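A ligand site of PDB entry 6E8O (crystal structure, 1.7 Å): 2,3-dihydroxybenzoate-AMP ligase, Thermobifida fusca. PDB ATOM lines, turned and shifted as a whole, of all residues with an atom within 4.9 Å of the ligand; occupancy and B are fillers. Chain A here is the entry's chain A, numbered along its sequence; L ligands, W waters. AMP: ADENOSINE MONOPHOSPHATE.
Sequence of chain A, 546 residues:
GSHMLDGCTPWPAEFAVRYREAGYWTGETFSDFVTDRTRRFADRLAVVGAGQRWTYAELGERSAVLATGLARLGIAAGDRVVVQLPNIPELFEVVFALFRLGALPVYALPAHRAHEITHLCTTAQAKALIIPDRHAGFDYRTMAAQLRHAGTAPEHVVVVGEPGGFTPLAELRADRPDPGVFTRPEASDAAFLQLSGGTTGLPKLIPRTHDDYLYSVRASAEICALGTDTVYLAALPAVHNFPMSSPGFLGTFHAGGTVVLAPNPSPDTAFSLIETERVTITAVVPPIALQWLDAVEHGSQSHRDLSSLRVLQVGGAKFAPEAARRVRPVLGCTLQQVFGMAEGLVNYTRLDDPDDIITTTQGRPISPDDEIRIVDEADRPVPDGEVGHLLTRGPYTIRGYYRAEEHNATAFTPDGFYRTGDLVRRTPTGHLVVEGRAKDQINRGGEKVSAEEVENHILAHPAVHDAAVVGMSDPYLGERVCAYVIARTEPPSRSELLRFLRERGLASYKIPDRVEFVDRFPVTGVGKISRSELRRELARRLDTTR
A nitrogen (N1) of the ligand lies close to the backbone carbonyl oxygen (O) of Ala 317.
The backbone carbonyl oxygen (O) of Gly 340 lies close to an oxygen (O1P) of the ligand (3.3 Å).
CA of Gly 315 touches N6 of the ligand, 3.9 Å away.
N of Lys 318 touches C2 of the ligand, 3.4 Å away.
CA of Phe 339 touches N7 of the ligand, at 3.5 Å.
Met 341 touches the ligand (CA to O1P, 3.6 Å).
Gln 362 touches the ligand (CG to N6, 3.7 Å).
Val 434 touches the ligand.
Asn 443 touches the ligand (ND2 to C1', 3.9 Å).
Hydrophobic or aromatic side chains that line the ligand: His 240, Phe 339, Met 341, Ala 342 and Val 434.
Of the 23 residues printed, 16 come within 4 Å of the ligand.
The backbone carbonyl oxygen (O) of Val 338 lies within hydrogen-bond range of a nitrogen (N6) of the ligand.
An oxygen (O2P) of the ligand lies within salt-bridge range of the side-chain amino group (NZ) of Lys 448 (3.1 Å).
An oxygen (O2') of the ligand sits at hydrogen-bond distance from the side-chain carboxylate of Asp 422 (2.8 Å).
A ring nitrogen (NE2) of His 240 is in hydrogen-bond range of an oxygen (O2P) of the ligand, at 2.9 Å.
The side-chain amino group (NZ) of Lys 439 lies within hydrogen-bond range of an oxygen (O3') of the ligand.
N of Gly 316 is in hydrogen-bond range of N7 of the ligand.
N of Ala 342 is in hydrogen-bond range of O3P of the ligand.
Water W7 lies within hydrogen-bond range of O2' of the ligand (2.5 Å), NE of Arg 437 (2.8 Å), OE1 of Gln 441 (2.9 Å) and ND2 of Asn 443 (3.3 Å).
Water W5 lies within hydrogen-bond range of an oxygen (O3P) of the ligand (2.8 Å), the backbone NH of Gly 197 (2.9 Å) and the side-chain carboxylate of Glu 343 (2.9 Å).
Water W1 lies within hydrogen-bond range of the backbone carbonyl oxygen of Val 314 (2.8 Å) and a nitrogen (N6) of the ligand (3.1 Å).
Water W2 lies within hydrogen-bond range of OE1 of Glu 343, O3' of the ligand, NZ of Lys 439 and SD of Met 341.
Water W9 lies within hydrogen-bond range of OD1 of Asp 422 (2.8 Å), NE of Arg 437 (3.4 Å) and O2' of the ligand (3.5 Å).
The side-chain carboxylate (OD1) of Asp 422 is in salt-bridge range of the side-chain amino group (NZ) of Lys 439 (3.7 Å).
O of Gly 446 sits at hydrogen-bond distance from NZ of Lys 448, 2.8 Å away.
The side-chain amino group (NZ) of Lys 439 lies within hydrogen-bond range of the backbone carbonyl oxygen (O) of Thr 420, at 2.8 Å.
The side-chain hydroxyl of Thr 420 lies within hydrogen-bond range of the backbone NH of Asp 422 (3.1 Å).
The side-chain amino group of Lys 318 is in hydrogen-bond range of the backbone carbonyl oxygen of Val 434 (2.8 Å).
The backbone carbonyl oxygen of Gly 316 is in hydrogen-bond range of the side-chain amide nitrogen of Asn 443 (3.1 Å).
The backbone NH of Gly 446 lies within hydrogen-bond range of the side-chain amide oxygen of Asn 443, 2.8 Å away.
O of Gly 316 is in hydrogen-bond range of NZ of Lys 448 (3.4 Å).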
ATOM      1  N   GLY A 197     -25.245  -6.385  14.629  1.00  0.00           N
ATOM      2  CA  GLY A 197     -25.620  -7.302  15.690  1.00  0.00           C
ATOM      3  C   GLY A 197     -27.083  -7.718  15.643  1.00  0.00           C
ATOM      4  O   GLY A 197     -27.431  -8.853  15.977  1.00  0.00           O
ATOM      5  N   HIS A 240     -15.587 -11.832  11.279  1.00  0.00           N
ATOM      6  CA  HIS A 240     -16.206 -10.854  12.145  1.00  0.00           C
ATOM      7  C   HIS A 240     -15.330  -9.607  12.235  1.00  0.00           C
ATOM      8  O   HIS A 240     -14.095  -9.678  12.129  1.00  0.00           O
ATOM      9  CB  HIS A 240     -16.476 -11.435  13.535  1.00  0.00           C
ATOM     10  CG  HIS A 240     -17.180 -10.485  14.456  1.00  0.00           C
ATOM     11  ND1 HIS A 240     -16.493  -9.614  15.287  1.00  0.00           N
ATOM     12  CD2 HIS A 240     -18.497 -10.257  14.667  1.00  0.00           C
ATOM     13  CE1 HIS A 240     -17.371  -8.902  15.973  1.00  0.00           C
ATOM     14  NE2 HIS A 240     -18.584  -9.276  15.622  1.00  0.00           N
ATOM     15  N   VAL A 314      -9.436  -8.788  24.433  1.00  0.00           N
ATOM     16  CA  VAL A 314     -10.732  -9.293  24.863  1.00  0.00           C
ATOM     17  C   VAL A 314     -11.783  -8.221  24.564  1.00  0.00           C
ATOM     18  O   VAL A 314     -11.639  -7.073  24.995  1.00  0.00           O
ATOM     19  CB  VAL A 314     -10.740  -9.656  26.353  1.00  0.00           C
ATOM     20  CG1 VAL A 314     -12.099 -10.241  26.736  1.00  0.00           C
ATOM     21  CG2 VAL A 314      -9.602 -10.627  26.681  1.00  0.00           C
ATOM     22  N   GLY A 315     -12.837  -8.609  23.851  1.00  0.00           N
ATOM     23  CA  GLY A 315     -13.888  -7.684  23.492  1.00  0.00           C
ATOM     24  C   GLY A 315     -15.125  -8.397  23.001  1.00  0.00           C
ATOM     25  O   GLY A 315     -15.241  -9.620  23.088  1.00  0.00           O
ATOM     26  N   GLY A 316     -16.060  -7.604  22.473  1.00  0.00           N
ATOM     27  CA  GLY A 316     -17.330  -8.085  21.986  1.00  0.00           C
ATOM     28  C   GLY A 316     -18.415  -8.143  23.045  1.00  0.00           C
ATOM     29  O   GLY A 316     -19.606  -8.100  22.717  1.00  0.00           O
ATOM     30  N   ALA A 317     -18.022  -8.225  24.321  1.00  0.00           N
ATOM     31  CA  ALA A 317     -18.934  -8.236  25.455  1.00  0.00           C
ATOM     32  C   ALA A 317     -18.136  -7.773  26.668  1.00  0.00           C
ATOM     33  O   ALA A 317     -16.914  -7.673  26.637  1.00  0.00           O
ATOM     34  CB  ALA A 317     -19.531  -9.630  25.675  1.00  0.00           C
ATOM     35  N   LYS A 318     -18.860  -7.476  27.749  1.00  0.00           N
ATOM     36  CA  LYS A 318     -18.241  -6.924  28.951  1.00  0.00           C
ATOM     37  C   LYS A 318     -17.290  -7.933  29.592  1.00  0.00           C
ATOM     38  O   LYS A 318     -17.631  -9.103  29.759  1.00  0.00           O
ATOM     39  CB  LYS A 318     -19.329  -6.499  29.942  1.00  0.00           C
ATOM     40  CG  LYS A 318     -18.787  -5.917  31.226  1.00  0.00           C
ATOM     41  CD  LYS A 318     -18.192  -4.546  31.015  1.00  0.00           C
ATOM     42  CE  LYS A 318     -17.823  -3.914  32.348  1.00  0.00           C
ATOM     43  NZ  LYS A 318     -17.580  -2.461  32.222  1.00  0.00           N
ATOM     44  N   VAL A 338     -11.072  -4.208  23.981  1.00  0.00           N
ATOM     45  CA  VAL A 338     -11.502  -3.691  22.684  1.00  0.00           C
ATOM     46  C   VAL A 338     -13.021  -3.610  22.703  1.00  0.00           C
ATOM     47  O   VAL A 338     -13.699  -4.643  22.729  1.00  0.00           O
ATOM     48  CB  VAL A 338     -11.021  -4.558  21.514  1.00  0.00           C
ATOM     49  CG1 VAL A 338     -11.314  -3.869  20.189  1.00  0.00           C
ATOM     50  CG2 VAL A 338      -9.549  -4.891  21.661  1.00  0.00           C
ATOM     51  N   PHE A 339     -13.547  -2.397  22.641  1.00  0.00           N
ATOM     52  CA  PHE A 339     -14.988  -2.149  22.574  1.00  0.00           C
ATOM     53  C   PHE A 339     -15.250  -1.503  21.213  1.00  0.00           C
ATOM     54  O   PHE A 339     -14.947  -0.322  21.001  1.00  0.00           O
ATOM     55  CB  PHE A 339     -15.420  -1.267  23.761  1.00  0.00           C
ATOM     56  CG  PHE A 339     -16.753  -0.583  23.583  1.00  0.00           C
ATOM     57  CD1 PHE A 339     -17.813  -1.227  22.978  1.00  0.00           C
ATOM     58  CD2 PHE A 339     -16.943   0.698  24.074  1.00  0.00           C
ATOM     59  CE1 PHE A 339     -19.038  -0.593  22.828  1.00  0.00           C
ATOM     60  CE2 PHE A 339     -18.162   1.333  23.937  1.00  0.00           C
ATOM     61  CZ  PHE A 339     -19.212   0.693  23.312  1.00  0.00           C
ATOM     62  N   GLY A 340     -15.797  -2.280  20.293  1.00  0.00           N
ATOM     63  CA  GLY A 340     -16.025  -1.809  18.942  1.00  0.00           C
ATOM     64  C   GLY A 340     -17.329  -2.365  18.402  1.00  0.00           C
ATOM     65  O   GLY A 340     -18.025  -3.137  19.064  1.00  0.00           O
ATOM     66  N   MET A 341     -17.664  -1.953  17.179  1.00  0.00           N
ATOM     67  CA  MET A 341     -18.920  -2.363  16.584  1.00  0.00           C
ATOM     68  C   MET A 341     -18.758  -2.406  15.074  1.00  0.00           C
ATOM     69  O   MET A 341     -17.910  -1.701  14.506  1.00  0.00           O
ATOM     70  CB  MET A 341     -20.061  -1.418  16.983  1.00  0.00           C
ATOM     71  CG  MET A 341     -19.765   0.052  16.755  1.00  0.00           C
ATOM     72  SD  MET A 341     -20.621   1.133  17.925  1.00  0.00           S
ATOM     73  CE  MET A 341     -19.650   0.864  19.411  1.00  0.00           C
ATOM     74  N   ALA A 342     -19.561  -3.254  14.438  1.00  0.00           N
ATOM     75  CA  ALA A 342     -19.493  -3.389  12.989  1.00  0.00           C
ATOM     76  C   ALA A 342     -19.864  -2.091  12.269  1.00  0.00           C
ATOM     77  O   ALA A 342     -19.462  -1.889  11.128  1.00  0.00           O
ATOM     78  CB  ALA A 342     -20.401  -4.527  12.523  1.00  0.00           C
ATOM     79  N   GLU A 343     -20.612  -1.206  12.940  1.00  0.00           N
ATOM     80  CA  GLU A 343     -21.026   0.064  12.365  1.00  0.00           C
ATOM     81  C   GLU A 343     -19.906   1.094  12.329  1.00  0.00           C
ATOM     82  O   GLU A 343     -20.043   2.105  11.629  1.00  0.00           O
ATOM     83  CB  GLU A 343     -22.222   0.643  13.131  1.00  0.00           C
ATOM     84  CG  GLU A 343     -23.547  -0.086  12.907  1.00  0.00           C
ATOM     85  CD  GLU A 343     -23.752  -1.252  13.862  1.00  0.00           C
ATOM     86  OE1 GLU A 343     -22.819  -1.591  14.626  1.00  0.00           O
ATOM     87  OE2 GLU A 343     -24.856  -1.850  13.845  1.00  0.00           O
ATOM     88  N   GLN A 362     -12.890   0.010  28.937  1.00  0.00           N
ATOM     89  CA  GLN A 362     -12.996  -0.615  27.616  1.00  0.00           C
ATOM     90  C   GLN A 362     -12.330   0.218  26.522  1.00  0.00           C
ATOM     91  O   GLN A 362     -12.643   0.040  25.336  1.00  0.00           O
ATOM     92  CB  GLN A 362     -14.462  -0.885  27.279  1.00  0.00           C
ATOM     93  CG  GLN A 362     -15.034  -2.132  27.922  1.00  0.00           C
ATOM     94  CD  GLN A 362     -15.179  -2.003  29.430  1.00  0.00           C
ATOM     95  OE1 GLN A 362     -16.000  -1.237  29.918  1.00  0.00           O
ATOM     96  NE2 GLN A 362     -14.381  -2.759  30.170  1.00  0.00           N
ATOM     97  N   THR A 420     -25.503   4.133  19.168  1.00  0.00           N
ATOM     98  CA  THR A 420     -24.909   2.806  19.379  1.00  0.00           C
ATOM     99  C   THR A 420     -25.835   1.875  20.150  1.00  0.00           C
ATOM    100  O   THR A 420     -25.752   0.651  19.997  1.00  0.00           O
ATOM    101  CB  THR A 420     -23.580   2.900  20.125  1.00  0.00           C
ATOM    102  OG1 THR A 420     -23.813   3.294  21.483  1.00  0.00           O
ATOM    103  CG2 THR A 420     -22.639   3.892  19.455  1.00  0.00           C
ATOM    104  N   ASP A 422     -25.596   1.696  23.411  1.00  0.00           N
ATOM    105  CA  ASP A 422     -24.843   1.346  24.602  1.00  0.00           C
ATOM    106  C   ASP A 422     -24.963   2.435  25.648  1.00  0.00           C
ATOM    107  O   ASP A 422     -25.090   3.626  25.332  1.00  0.00           O
ATOM    108  CB  ASP A 422     -23.373   1.105  24.257  1.00  0.00           C
ATOM    109  CG  ASP A 422     -23.195  -0.008  23.263  1.00  0.00           C
ATOM    110  OD1 ASP A 422     -23.785  -1.084  23.475  1.00  0.00           O
ATOM    111  OD2 ASP A 422     -22.492   0.208  22.262  1.00  0.00           O
ATOM    112  N   VAL A 434     -18.226   0.543  29.656  1.00  0.00           N
ATOM    113  CA  VAL A 434     -19.536   0.066  29.226  1.00  0.00           C
ATOM    114  C   VAL A 434     -20.285  -0.405  30.463  1.00  0.00           C
ATOM    115  O   VAL A 434     -19.860  -1.349  31.144  1.00  0.00           O
ATOM    116  CB  VAL A 434     -19.418  -1.057  28.182  1.00  0.00           C
ATOM    117  CG1 VAL A 434     -20.793  -1.430  27.657  1.00  0.00           C
ATOM    118  CG2 VAL A 434     -18.488  -0.625  27.049  1.00  0.00           C
ATOM    119  N   ARG A 437     -26.935  -1.428  28.546  1.00  0.00           N
ATOM    120  CA  ARG A 437     -27.429  -1.413  27.177  1.00  0.00           C
ATOM    121  C   ARG A 437     -28.845  -0.836  27.148  1.00  0.00           C
ATOM    122  O   ARG A 437     -29.633  -1.074  28.064  1.00  0.00           O
ATOM    123  CB  ARG A 437     -27.426  -2.817  26.572  1.00  0.00           C
ATOM    124  CG  ARG A 437     -27.419  -2.830  25.064  1.00  0.00           C
ATOM    125  CD  ARG A 437     -27.240  -4.239  24.549  1.00  0.00           C
ATOM    126  NE  ARG A 437     -26.169  -4.915  25.277  1.00  0.00           N
ATOM    127  CZ  ARG A 437     -26.362  -5.965  26.068  1.00  0.00           C
ATOM    128  NH1 ARG A 437     -27.571  -6.472  26.232  1.00  0.00           N
ATOM    129  NH2 ARG A 437     -25.319  -6.510  26.698  1.00  0.00           N
ATOM    130  N   LYS A 439     -30.411  -0.646  23.631  1.00  0.00           N
ATOM    131  CA  LYS A 439     -30.993  -1.359  22.509  1.00  0.00           C
ATOM    132  C   LYS A 439     -31.509  -2.726  22.948  1.00  0.00           C
ATOM    133  O   LYS A 439     -30.942  -3.374  23.839  1.00  0.00           O
ATOM    134  CB  LYS A 439     -29.963  -1.544  21.393  1.00  0.00           C
ATOM    135  CG  LYS A 439     -28.703  -2.303  21.801  1.00  0.00           C
ATOM    136  CD  LYS A 439     -27.656  -2.251  20.697  1.00  0.00           C
ATOM    137  CE  LYS A 439     -26.254  -2.311  21.279  1.00  0.00           C
ATOM    138  NZ  LYS A 439     -25.200  -2.106  20.240  1.00  0.00           N
ATOM    139  N   GLN A 441     -31.359  -6.119  22.692  1.00  0.00           N
ATOM    140  CA  GLN A 441     -30.370  -7.056  22.160  1.00  0.00           C
ATOM    141  C   GLN A 441     -29.753  -7.818  23.319  1.00  0.00           C
ATOM    142  O   GLN A 441     -29.235  -7.195  24.255  1.00  0.00           O
ATOM    143  CB  GLN A 441     -29.301  -6.329  21.357  1.00  0.00           C
ATOM    144  CG  GLN A 441     -28.179  -7.229  20.863  1.00  0.00           C
ATOM    145  CD  GLN A 441     -27.081  -6.442  20.162  1.00  0.00           C
ATOM    146  OE1 GLN A 441     -26.118  -5.994  20.808  1.00  0.00           O
ATOM    147  NE2 GLN A 441     -27.205  -6.275  18.853  1.00  0.00           N
ATOM    148  N   ASN A 443     -26.742 -10.131  24.550  1.00  0.00           N
ATOM    149  CA  ASN A 443     -25.349 -10.318  24.147  1.00  0.00           C
ATOM    150  C   ASN A 443     -24.859 -11.600  24.819  1.00  0.00           C
ATOM    151  O   ASN A 443     -24.452 -11.594  25.986  1.00  0.00           O
ATOM    152  CB  ASN A 443     -24.495  -9.110  24.544  1.00  0.00           C
ATOM    153  CG  ASN A 443     -23.086  -9.193  24.007  1.00  0.00           C
ATOM    154  OD1 ASN A 443     -22.609 -10.274  23.644  1.00  0.00           O
ATOM    155  ND2 ASN A 443     -22.395  -8.052  23.957  1.00  0.00           N
ATOM    156  N   GLY A 446     -20.730 -12.297  23.299  1.00  0.00           N
ATOM    157  CA  GLY A 446     -20.254 -11.697  22.079  1.00  0.00           C
ATOM    158  C   GLY A 446     -21.129 -11.943  20.867  1.00  0.00           C
ATOM    159  O   GLY A 446     -20.994 -11.233  19.858  1.00  0.00           O
ATOM    160  N   LYS A 448     -24.799 -11.724  19.271  1.00  0.00           N
ATOM    161  CA  LYS A 448     -25.944 -10.853  19.526  1.00  0.00           C
ATOM    162  C   LYS A 448     -27.250 -11.531  19.121  1.00  0.00           C
ATOM    163  O   LYS A 448     -27.341 -12.115  18.033  1.00  0.00           O
ATOM    164  CB  LYS A 448     -25.778  -9.534  18.775  1.00  0.00           C
ATOM    165  CG  LYS A 448     -24.384  -8.899  18.897  1.00  0.00           C
ATOM    166  CD  LYS A 448     -23.979  -8.687  20.344  1.00  0.00           C
ATOM    167  CE  LYS A 448     -22.725  -7.813  20.474  1.00  0.00           C
ATOM    168  NZ  LYS A 448     -21.486  -8.433  19.914  1.00  0.00           N
HETATM  169  P   AMP L   1     -20.394  -6.289  16.990  1.00  0.00           P
HETATM  170  O1P AMP L   1     -19.003  -5.847  17.382  1.00  0.00           O
HETATM  171  O2P AMP L   1     -20.622  -7.788  17.016  1.00  0.00           O
HETATM  172  O3P AMP L   1     -20.952  -5.578  15.780  1.00  0.00           O
HETATM  173  O5' AMP L   1     -21.320  -5.733  18.145  1.00  0.00           O
HETATM  174  C5' AMP L   1     -21.086  -4.473  18.744  1.00  0.00           C
HETATM  175  C4' AMP L   1     -21.670  -4.398  20.129  1.00  0.00           C
HETATM  176  O4' AMP L   1     -20.999  -5.351  21.001  1.00  0.00           O
HETATM  177  C3' AMP L   1     -21.507  -3.067  20.837  1.00  0.00           C
HETATM  178  O3' AMP L   1     -22.467  -2.119  20.420  1.00  0.00           O
HETATM  179  C2' AMP L   1     -21.620  -3.461  22.307  1.00  0.00           C
HETATM  180  O2' AMP L   1     -22.978  -3.646  22.699  1.00  0.00           O
HETATM  181  C1' AMP L   1     -20.939  -4.834  22.306  1.00  0.00           C
HETATM  182  N9  AMP L   1     -19.523  -4.773  22.716  1.00  0.00           N
HETATM  183  C8  AMP L   1     -18.465  -4.868  21.890  1.00  0.00           C
HETATM  184  N7  AMP L   1     -17.311  -4.796  22.600  1.00  0.00           N
HETATM  185  C5  AMP L   1     -17.628  -4.661  23.900  1.00  0.00           C
HETATM  186  C6  AMP L   1     -16.905  -4.521  25.168  1.00  0.00           C
HETATM  187  N6  AMP L   1     -15.562  -4.524  25.168  1.00  0.00           N
HETATM  188  N1  AMP L   1     -17.627  -4.397  26.306  1.00  0.00           N
HETATM  189  C2  AMP L   1     -18.963  -4.400  26.303  1.00  0.00           C
HETATM  190  N3  AMP L   1     -19.691  -4.523  25.177  1.00  0.00           N
HETATM  191  C4  AMP L   1     -19.098  -4.650  23.975  1.00  0.00           C
HETATM  192  O   HOH W   1     -13.380  -5.880  26.903  1.00  0.00           O
HETATM  193  O   HOH W   2     -23.544  -0.840  17.588  1.00  0.00           O
HETATM  194  O   HOH W   3     -16.621  -5.191  16.086  1.00  0.00           O
HETATM  195  O   HOH W   4     -22.289  -9.273  15.886  1.00  0.00           O
HETATM  196  O   HOH W   5     -23.477  -4.307  15.462  1.00  0.00           O
HETATM  197  O   HOH W   6     -17.073  -6.549  18.974  1.00  0.00           O
HETATM  198  O   HOH W   7     -24.463  -5.614  23.207  1.00  0.00           O
HETATM  199  O   HOH W   8     -21.186  -7.724  13.510  1.00  0.00           O
HETATM  200  O   HOH W   9     -23.856  -2.511  25.883  1.00  0.00           O
HETATM  201  O   HOH W  10     -22.262  -4.792  26.056  1.00  0.00           O
